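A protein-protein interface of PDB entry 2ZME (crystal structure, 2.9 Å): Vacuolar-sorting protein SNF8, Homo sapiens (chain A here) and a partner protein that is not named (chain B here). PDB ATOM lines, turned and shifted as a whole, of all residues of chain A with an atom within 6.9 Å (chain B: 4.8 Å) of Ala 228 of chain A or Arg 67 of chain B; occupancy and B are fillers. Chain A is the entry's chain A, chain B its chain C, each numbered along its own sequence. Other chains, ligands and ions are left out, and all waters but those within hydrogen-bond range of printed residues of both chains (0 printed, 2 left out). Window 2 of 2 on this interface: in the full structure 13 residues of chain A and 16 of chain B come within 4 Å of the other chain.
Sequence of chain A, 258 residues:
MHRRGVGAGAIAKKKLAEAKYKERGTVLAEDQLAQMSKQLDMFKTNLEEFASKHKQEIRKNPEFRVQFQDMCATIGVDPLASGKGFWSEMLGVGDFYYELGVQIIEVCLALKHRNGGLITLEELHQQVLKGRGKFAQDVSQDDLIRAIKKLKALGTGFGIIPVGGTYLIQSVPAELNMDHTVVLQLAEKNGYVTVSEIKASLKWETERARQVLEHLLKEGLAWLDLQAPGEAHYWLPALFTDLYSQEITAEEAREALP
OD1 of Asp 225 of chain A lies within salt-bridge range of NH1 of Arg 67 of chain B (2.5 Å). O of Phe 17 of chain B is in hydrogen-bond range of NE2 of Gln 227 of chain A, 2.9 Å away. The side-chain amide nitrogen (NE2) of Gln 227 of chain A is in hydrogen-bond range of the backbone carbonyl oxygen (O) of Lys 68 of chain B, at 2.9 Å.
OD2 of Asp 225 of chain A sits at hydrogen-bond distance from N of Gln 227 of chain A (3.0 Å). The backbone NH of Asp 225 of chain A lies within hydrogen-bond range of the backbone carbonyl oxygen of His 233 of chain A (2.8 Å). The indole nitrogen (NE1) of Trp 235 of chain A is in hydrogen-bond range of the side-chain carboxylate (OD1) of Asp 225 of chain A, 2.9 Å away. N of Asn 62 of chain B lies within hydrogen-bond range of O of Arg 67 of chain B (2.8 Å). O of Leu 65 of chain B lies close to NE of Arg 67 of chain B, 3.5 Å away.
Pro 14 of chain B touches Asp 225 of chain A. Arg 67 of chain B touches Gln 227 of chain A (CA to OE1, 3.4 Å). Ala 228 of chain A touches Arg 67 of chain B (N to NH1, 3.8 Å). Trp 235 of chain A touches Pro 14 of chain B (CZ2 to CG, 3.7 Å).
Of the printed residues of chain B, Gln 227 of chain A touches Phe 17, Arg 67 and Lys 68. Ala 228 of chain A touches just one residue of chain B: Arg 67 (3.8 Å). Printed residues of chain B within 4 Å of Trp 235 of chain A: Pro 14. Asn 61 of chain B touches none of the printed residues of chain A. Printed residues of chain A within 4 Å of Arg 67 of chain B: Asp 225, Gln 227 and Ala 228. Of the printed residues of chain A, Lys 68 of chain B touches Gln 227 (2.9 Å). The nearest residue of chain A that does not touch Arg 67 of chain B is Pro 229 of chain A (4.4 Å).
Of the 10 printed residues of chain B, 4 touch a printed residue of chain A. Printed residues of chain B that touch a printed residue of chain A: Pro 14, Phe 17, Arg 67 and Lys 68. Hydrophobic or aromatic side chains of chain B that line the printed part of chain A: Pro 14. Of the 11 printed residues of chain A, 4 touch a printed residue of chain B. Among the printed residues, Asp or Glu carboxylates within 4 Å of a Lys or Arg side-chain nitrogen of the other chain: Asp 225 of chain A with Arg 67 of chain B.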
ATOM      1  N   THR A 194      37.366   0.055 -19.697  1.00  0.00           N
ATOM      2  CA  THR A 194      37.958   0.230 -21.003  1.00  0.00           C
ATOM      3  C   THR A 194      39.427   0.528 -20.795  1.00  0.00           C
ATOM      4  O   THR A 194      39.804   1.128 -19.786  1.00  0.00           O
ATOM      5  CB  THR A 194      37.153   1.374 -21.693  1.00  0.00           C
ATOM      6  OG1 THR A 194      36.365   0.831 -22.776  1.00  0.00           O
ATOM      7  CG2 THR A 194      38.012   2.541 -22.185  1.00  0.00           C
ATOM      8  N   ASP A 225      33.889  -7.225 -25.031  1.00  0.00           N
ATOM      9  CA  ASP A 225      32.894  -6.709 -25.946  1.00  0.00           C
ATOM     10  C   ASP A 225      33.507  -5.874 -27.090  1.00  0.00           C
ATOM     11  O   ASP A 225      34.012  -4.772 -26.818  1.00  0.00           O
ATOM     12  CB  ASP A 225      31.901  -5.853 -25.173  1.00  0.00           C
ATOM     13  CG  ASP A 225      30.951  -5.091 -26.086  1.00  0.00           C
ATOM     14  OD1 ASP A 225      30.342  -4.103 -25.605  1.00  0.00           O
ATOM     15  OD2 ASP A 225      30.825  -5.479 -27.282  1.00  0.00           O
ATOM     16  N   LEU A 226      33.419  -6.367 -28.343  1.00  0.00           N
ATOM     17  CA  LEU A 226      34.046  -5.718 -29.535  1.00  0.00           C
ATOM     18  C   LEU A 226      33.060  -4.955 -30.425  1.00  0.00           C
ATOM     19  O   LEU A 226      33.256  -4.850 -31.623  1.00  0.00           O
ATOM     20  CB  LEU A 226      34.797  -6.734 -30.409  1.00  0.00           C
ATOM     21  CG  LEU A 226      35.961  -7.515 -29.793  1.00  0.00           C
ATOM     22  CD1 LEU A 226      36.321  -8.739 -30.584  1.00  0.00           C
ATOM     23  CD2 LEU A 226      37.160  -6.670 -29.606  1.00  0.00           C
ATOM     24  N   GLN A 227      31.983  -4.435 -29.848  1.00  0.00           N
ATOM     25  CA  GLN A 227      30.964  -3.736 -30.624  1.00  0.00           C
ATOM     26  C   GLN A 227      30.553  -2.481 -29.899  1.00  0.00           C
ATOM     27  O   GLN A 227      29.529  -1.900 -30.216  1.00  0.00           O
ATOM     28  CB  GLN A 227      29.739  -4.642 -30.909  1.00  0.00           C
ATOM     29  CG  GLN A 227      30.051  -5.848 -31.757  1.00  0.00           C
ATOM     30  CD  GLN A 227      28.900  -6.804 -31.903  1.00  0.00           C
ATOM     31  OE1 GLN A 227      27.728  -6.391 -31.905  1.00  0.00           O
ATOM     32  NE2 GLN A 227      29.218  -8.127 -32.041  1.00  0.00           N
ATOM     33  N   ALA A 228      31.335  -2.034 -28.927  1.00  0.00           N
ATOM     34  CA  ALA A 228      30.978  -0.780 -28.269  1.00  0.00           C
ATOM     35  C   ALA A 228      31.485   0.375 -29.120  1.00  0.00           C
ATOM     36  O   ALA A 228      32.199   0.152 -30.096  1.00  0.00           O
ATOM     37  CB  ALA A 228      31.563  -0.703 -26.896  1.00  0.00           C
ATOM     38  N   PRO A 229      31.075   1.619 -28.776  1.00  0.00           N
ATOM     39  CA  PRO A 229      31.580   2.775 -29.544  1.00  0.00           C
ATOM     40  C   PRO A 229      33.107   2.779 -29.677  1.00  0.00           C
ATOM     41  O   PRO A 229      33.583   2.232 -30.634  1.00  0.00           O
ATOM     42  CB  PRO A 229      31.016   3.980 -28.796  1.00  0.00           C
ATOM     43  CG  PRO A 229      29.709   3.427 -28.196  1.00  0.00           C
ATOM     44  CD  PRO A 229      30.089   2.029 -27.748  1.00  0.00           C
ATOM     45  N   GLY A 230      33.895   3.344 -28.787  1.00  0.00           N
ATOM     46  CA  GLY A 230      35.287   3.704 -29.228  1.00  0.00           C
ATOM     47  C   GLY A 230      36.375   2.629 -29.230  1.00  0.00           C
ATOM     48  O   GLY A 230      37.361   2.728 -29.969  1.00  0.00           O
ATOM     49  N   GLU A 231      36.199   1.624 -28.367  1.00  0.00           N
ATOM     50  CA  GLU A 231      37.075   0.480 -28.277  1.00  0.00           C
ATOM     51  C   GLU A 231      36.429  -0.697 -27.505  1.00  0.00           C
ATOM     52  O   GLU A 231      35.255  -0.621 -27.033  1.00  0.00           O
ATOM     53  CB  GLU A 231      38.399   0.892 -27.606  1.00  0.00           C
ATOM     54  CG  GLU A 231      38.374   0.963 -26.078  1.00  0.00           C
ATOM     55  CD  GLU A 231      39.244   2.072 -25.523  1.00  0.00           C
ATOM     56  OE1 GLU A 231      40.267   1.766 -24.836  1.00  0.00           O
ATOM     57  OE2 GLU A 231      38.908   3.256 -25.784  1.00  0.00           O
ATOM     58  N   ALA A 232      37.234  -1.766 -27.359  1.00  0.00           N
ATOM     59  CA  ALA A 232      36.905  -2.952 -26.567  1.00  0.00           C
ATOM     60  C   ALA A 232      36.504  -2.576 -25.182  1.00  0.00           C
ATOM     61  O   ALA A 232      37.283  -1.991 -24.446  1.00  0.00           O
ATOM     62  CB  ALA A 232      38.080  -3.836 -26.493  1.00  0.00           C
ATOM     63  N   HIS A 233      35.280  -2.924 -24.840  1.00  0.00           N
ATOM     64  CA  HIS A 233      34.759  -2.763 -23.507  1.00  0.00           C
ATOM     65  C   HIS A 233      34.792  -4.059 -22.809  1.00  0.00           C
ATOM     66  O   HIS A 233      34.655  -5.100 -23.426  1.00  0.00           O
ATOM     67  CB  HIS A 233      33.327  -2.335 -23.606  1.00  0.00           C
ATOM     68  CG  HIS A 233      33.188  -0.889 -23.905  1.00  0.00           C
ATOM     69  ND1 HIS A 233      34.036  -0.234 -24.775  1.00  0.00           N
ATOM     70  CD2 HIS A 233      32.332   0.042 -23.424  1.00  0.00           C
ATOM     71  CE1 HIS A 233      33.692   1.039 -24.824  1.00  0.00           C
ATOM     72  NE2 HIS A 233      32.664   1.232 -24.012  1.00  0.00           N
ATOM     73  N   TRP A 235      33.089  -5.942 -19.790  1.00  0.00           N
ATOM     74  CA  TRP A 235      31.966  -5.893 -18.891  1.00  0.00           C
ATOM     75  C   TRP A 235      32.124  -6.937 -17.819  1.00  0.00           C
ATOM     76  O   TRP A 235      32.486  -8.052 -18.133  1.00  0.00           O
ATOM     77  CB  TRP A 235      30.706  -6.212 -19.660  1.00  0.00           C
ATOM     78  CG  TRP A 235      30.390  -5.263 -20.731  1.00  0.00           C
ATOM     79  CD1 TRP A 235      31.057  -5.094 -21.904  1.00  0.00           C
ATOM     80  CD2 TRP A 235      29.292  -4.345 -20.753  1.00  0.00           C
ATOM     81  NE1 TRP A 235      30.440  -4.124 -22.663  1.00  0.00           N
ATOM     82  CE2 TRP A 235      29.358  -3.645 -21.971  1.00  0.00           C
ATOM     83  CE3 TRP A 235      28.275  -4.034 -19.858  1.00  0.00           C
ATOM     84  CZ2 TRP A 235      28.441  -2.646 -22.301  1.00  0.00           C
ATOM     85  CZ3 TRP A 235      27.375  -3.046 -20.197  1.00  0.00           C
ATOM     86  CH2 TRP A 235      27.464  -2.363 -21.396  1.00  0.00           C
ATOM     87  N   PRO B  14      25.569  -7.333 -23.377  1.00  0.00           N
ATOM     88  CA  PRO B  14      26.321  -7.000 -24.594  1.00  0.00           C
ATOM     89  C   PRO B  14      27.409  -8.003 -25.045  1.00  0.00           C
ATOM     90  O   PRO B  14      27.394  -8.415 -26.210  1.00  0.00           O
ATOM     91  CB  PRO B  14      26.884  -5.607 -24.297  1.00  0.00           C
ATOM     92  CG  PRO B  14      25.855  -4.993 -23.497  1.00  0.00           C
ATOM     93  CD  PRO B  14      25.373  -6.128 -22.556  1.00  0.00           C
ATOM     94  N   PHE B  17      27.491 -11.197 -27.447  1.00  0.00           N
ATOM     95  CA  PHE B  17      27.481 -11.050 -28.924  1.00  0.00           C
ATOM     96  C   PHE B  17      28.914 -11.040 -29.512  1.00  0.00           C
ATOM     97  O   PHE B  17      29.126 -10.627 -30.650  1.00  0.00           O
ATOM     98  CB  PHE B  17      26.630  -9.837 -29.345  1.00  0.00           C
ATOM     99  CG  PHE B  17      25.158 -10.015 -29.065  1.00  0.00           C
ATOM    100  CD1 PHE B  17      24.620  -9.666 -27.827  1.00  0.00           C
ATOM    101  CD2 PHE B  17      24.303 -10.577 -30.038  1.00  0.00           C
ATOM    102  CE1 PHE B  17      23.257  -9.865 -27.534  1.00  0.00           C
ATOM    103  CE2 PHE B  17      22.912 -10.783 -29.776  1.00  0.00           C
ATOM    104  CZ  PHE B  17      22.390 -10.416 -28.515  1.00  0.00           C
ATOM    105  N   PHE B  60      19.607 -13.340 -33.368  1.00  0.00           N
ATOM    106  CA  PHE B  60      20.998 -12.928 -33.333  1.00  0.00           C
ATOM    107  C   PHE B  60      21.170 -11.436 -33.410  1.00  0.00           C
ATOM    108  O   PHE B  60      22.293 -10.937 -33.358  1.00  0.00           O
ATOM    109  CB  PHE B  60      21.760 -13.564 -34.468  1.00  0.00           C
ATOM    110  CG  PHE B  60      21.801 -15.037 -34.401  1.00  0.00           C
ATOM    111  CD1 PHE B  60      21.198 -15.802 -35.385  1.00  0.00           C
ATOM    112  CD2 PHE B  60      22.442 -15.677 -33.347  1.00  0.00           C
ATOM    113  CE1 PHE B  60      21.240 -17.206 -35.352  1.00  0.00           C
ATOM    114  CE2 PHE B  60      22.485 -17.058 -33.274  1.00  0.00           C
ATOM    115  CZ  PHE B  60      21.877 -17.835 -34.293  1.00  0.00           C
ATOM    116  N   ASN B  61      20.082 -10.702 -33.532  1.00  0.00           N
ATOM    117  CA  ASN B  61      20.241  -9.275 -33.675  1.00  0.00           C
ATOM    118  C   ASN B  61      19.459  -8.545 -32.623  1.00  0.00           C
ATOM    119  O   ASN B  61      18.232  -8.491 -32.674  1.00  0.00           O
ATOM    120  CB  ASN B  61      19.844  -8.814 -35.075  1.00  0.00           C
ATOM    121  CG  ASN B  61      20.473  -7.491 -35.448  1.00  0.00           C
ATOM    122  OD1 ASN B  61      20.325  -7.006 -36.589  1.00  0.00           O
ATOM    123  ND2 ASN B  61      21.192  -6.889 -34.494  1.00  0.00           N
ATOM    124  N   ASN B  62      20.163  -7.996 -31.647  1.00  0.00           N
ATOM    125  CA  ASN B  62      19.472  -7.223 -30.671  1.00  0.00           C
ATOM    126  C   ASN B  62      19.560  -5.760 -30.986  1.00  0.00           C
ATOM    127  O   ASN B  62      20.531  -5.062 -30.644  1.00  0.00           O
ATOM    128  CB  ASN B  62      19.929  -7.504 -29.260  1.00  0.00           C
ATOM    129  CG  ASN B  62      19.019  -6.856 -28.247  1.00  0.00           C
ATOM    130  OD1 ASN B  62      18.760  -5.644 -28.293  1.00  0.00           O
ATOM    131  ND2 ASN B  62      18.496  -7.662 -27.346  1.00  0.00           N
ATOM    132  N   LEU B  65      19.807  -3.228 -27.946  1.00  0.00           N
ATOM    133  CA  LEU B  65      21.075  -3.418 -27.253  1.00  0.00           C
ATOM    134  C   LEU B  65      22.121  -3.023 -28.236  1.00  0.00           C
ATOM    135  O   LEU B  65      23.289  -2.910 -27.893  1.00  0.00           O
ATOM    136  CB  LEU B  65      21.317  -4.870 -26.904  1.00  0.00           C
ATOM    137  CG  LEU B  65      21.734  -5.074 -25.447  1.00  0.00           C
ATOM    138  CD1 LEU B  65      22.621  -6.345 -25.248  1.00  0.00           C
ATOM    139  CD2 LEU B  65      22.435  -3.827 -24.963  1.00  0.00           C
ATOM    140  N   GLN B  66      21.682  -2.851 -29.481  1.00  0.00           N
ATOM    141  CA  GLN B  66      22.563  -2.511 -30.553  1.00  0.00           C
ATOM    142  C   GLN B  66      23.765  -3.443 -30.590  1.00  0.00           C
ATOM    143  O   GLN B  66      24.895  -2.988 -30.561  1.00  0.00           O
ATOM    144  CB  GLN B  66      23.002  -1.066 -30.386  1.00  0.00           C
ATOM    145  CG  GLN B  66      22.428  -0.153 -31.429  1.00  0.00           C
ATOM    146  CD  GLN B  66      21.955   1.167 -30.862  1.00  0.00           C
ATOM    147  OE1 GLN B  66      21.240   1.919 -31.543  1.00  0.00           O
ATOM    148  NE2 GLN B  66      22.334   1.462 -29.615  1.00  0.00           N
ATOM    149  N   ARG B  67      23.511  -4.747 -30.620  1.00  0.00           N
ATOM    150  CA  ARG B  67      24.569  -5.759 -30.768  1.00  0.00           C
ATOM    151  C   ARG B  67      24.060  -6.916 -31.576  1.00  0.00           C
ATOM    152  O   ARG B  67      22.904  -7.323 -31.437  1.00  0.00           O
ATOM    153  CB  ARG B  67      25.014  -6.329 -29.421  1.00  0.00           C
ATOM    154  CG  ARG B  67      25.465  -5.329 -28.406  1.00  0.00           C
ATOM    155  CD  ARG B  67      26.762  -4.641 -28.795  1.00  0.00           C
ATOM    156  NE  ARG B  67      26.686  -3.212 -28.505  1.00  0.00           N
ATOM    157  CZ  ARG B  67      27.408  -2.571 -27.591  1.00  0.00           C
ATOM    158  NH1 ARG B  67      28.326  -3.188 -26.860  1.00  0.00           N
ATOM    159  NH2 ARG B  67      27.223  -1.264 -27.434  1.00  0.00           N
ATOM    160  N   LYS B  68      24.925  -7.469 -32.405  1.00  0.00           N
ATOM    161  CA  LYS B  68      24.533  -8.638 -33.185  1.00  0.00           C
ATOM    162  C   LYS B  68      25.651  -9.672 -33.242  1.00  0.00           C
ATOM    163  O   LYS B  68      26.842  -9.322 -33.157  1.00  0.00           O
ATOM    164  CB  LYS B  68      24.063  -8.238 -34.585  1.00  0.00           C
ATOM    165  CG  LYS B  68      25.026  -7.335 -35.347  1.00  0.00           C
ATOM    166  CD  LYS B  68      24.282  -6.422 -36.342  1.00  0.00           C
ATOM    167  CE  LYS B  68      23.562  -7.201 -37.476  1.00  0.00           C
ATOM    168  NZ  LYS B  68      24.503  -7.895 -38.428  1.00  0.00           N
ATOM    169  N   LEU B  69      25.254 -10.937 -33.341  1.00  0.00           N
ATOM    170  CA  LEU B  69      26.189 -12.041 -33.413  1.00  0.00           C
ATOM    171  C   LEU B  69      26.806 -12.029 -34.817  1.00  0.00           C
ATOM    172  O   LEU B  69      26.105 -12.249 -35.767  1.00  0.00           O
ATOM    173  CB  LEU B  69      25.452 -13.351 -33.188  1.00  0.00           C
ATOM    174  CG  LEU B  69      26.084 -14.429 -32.323  1.00  0.00           C
ATOM    175  CD1 LEU B  69      25.619 -15.806 -32.713  1.00  0.00           C
ATOM    176  CD2 LEU B  69      27.554 -14.393 -32.381  1.00  0.00           C
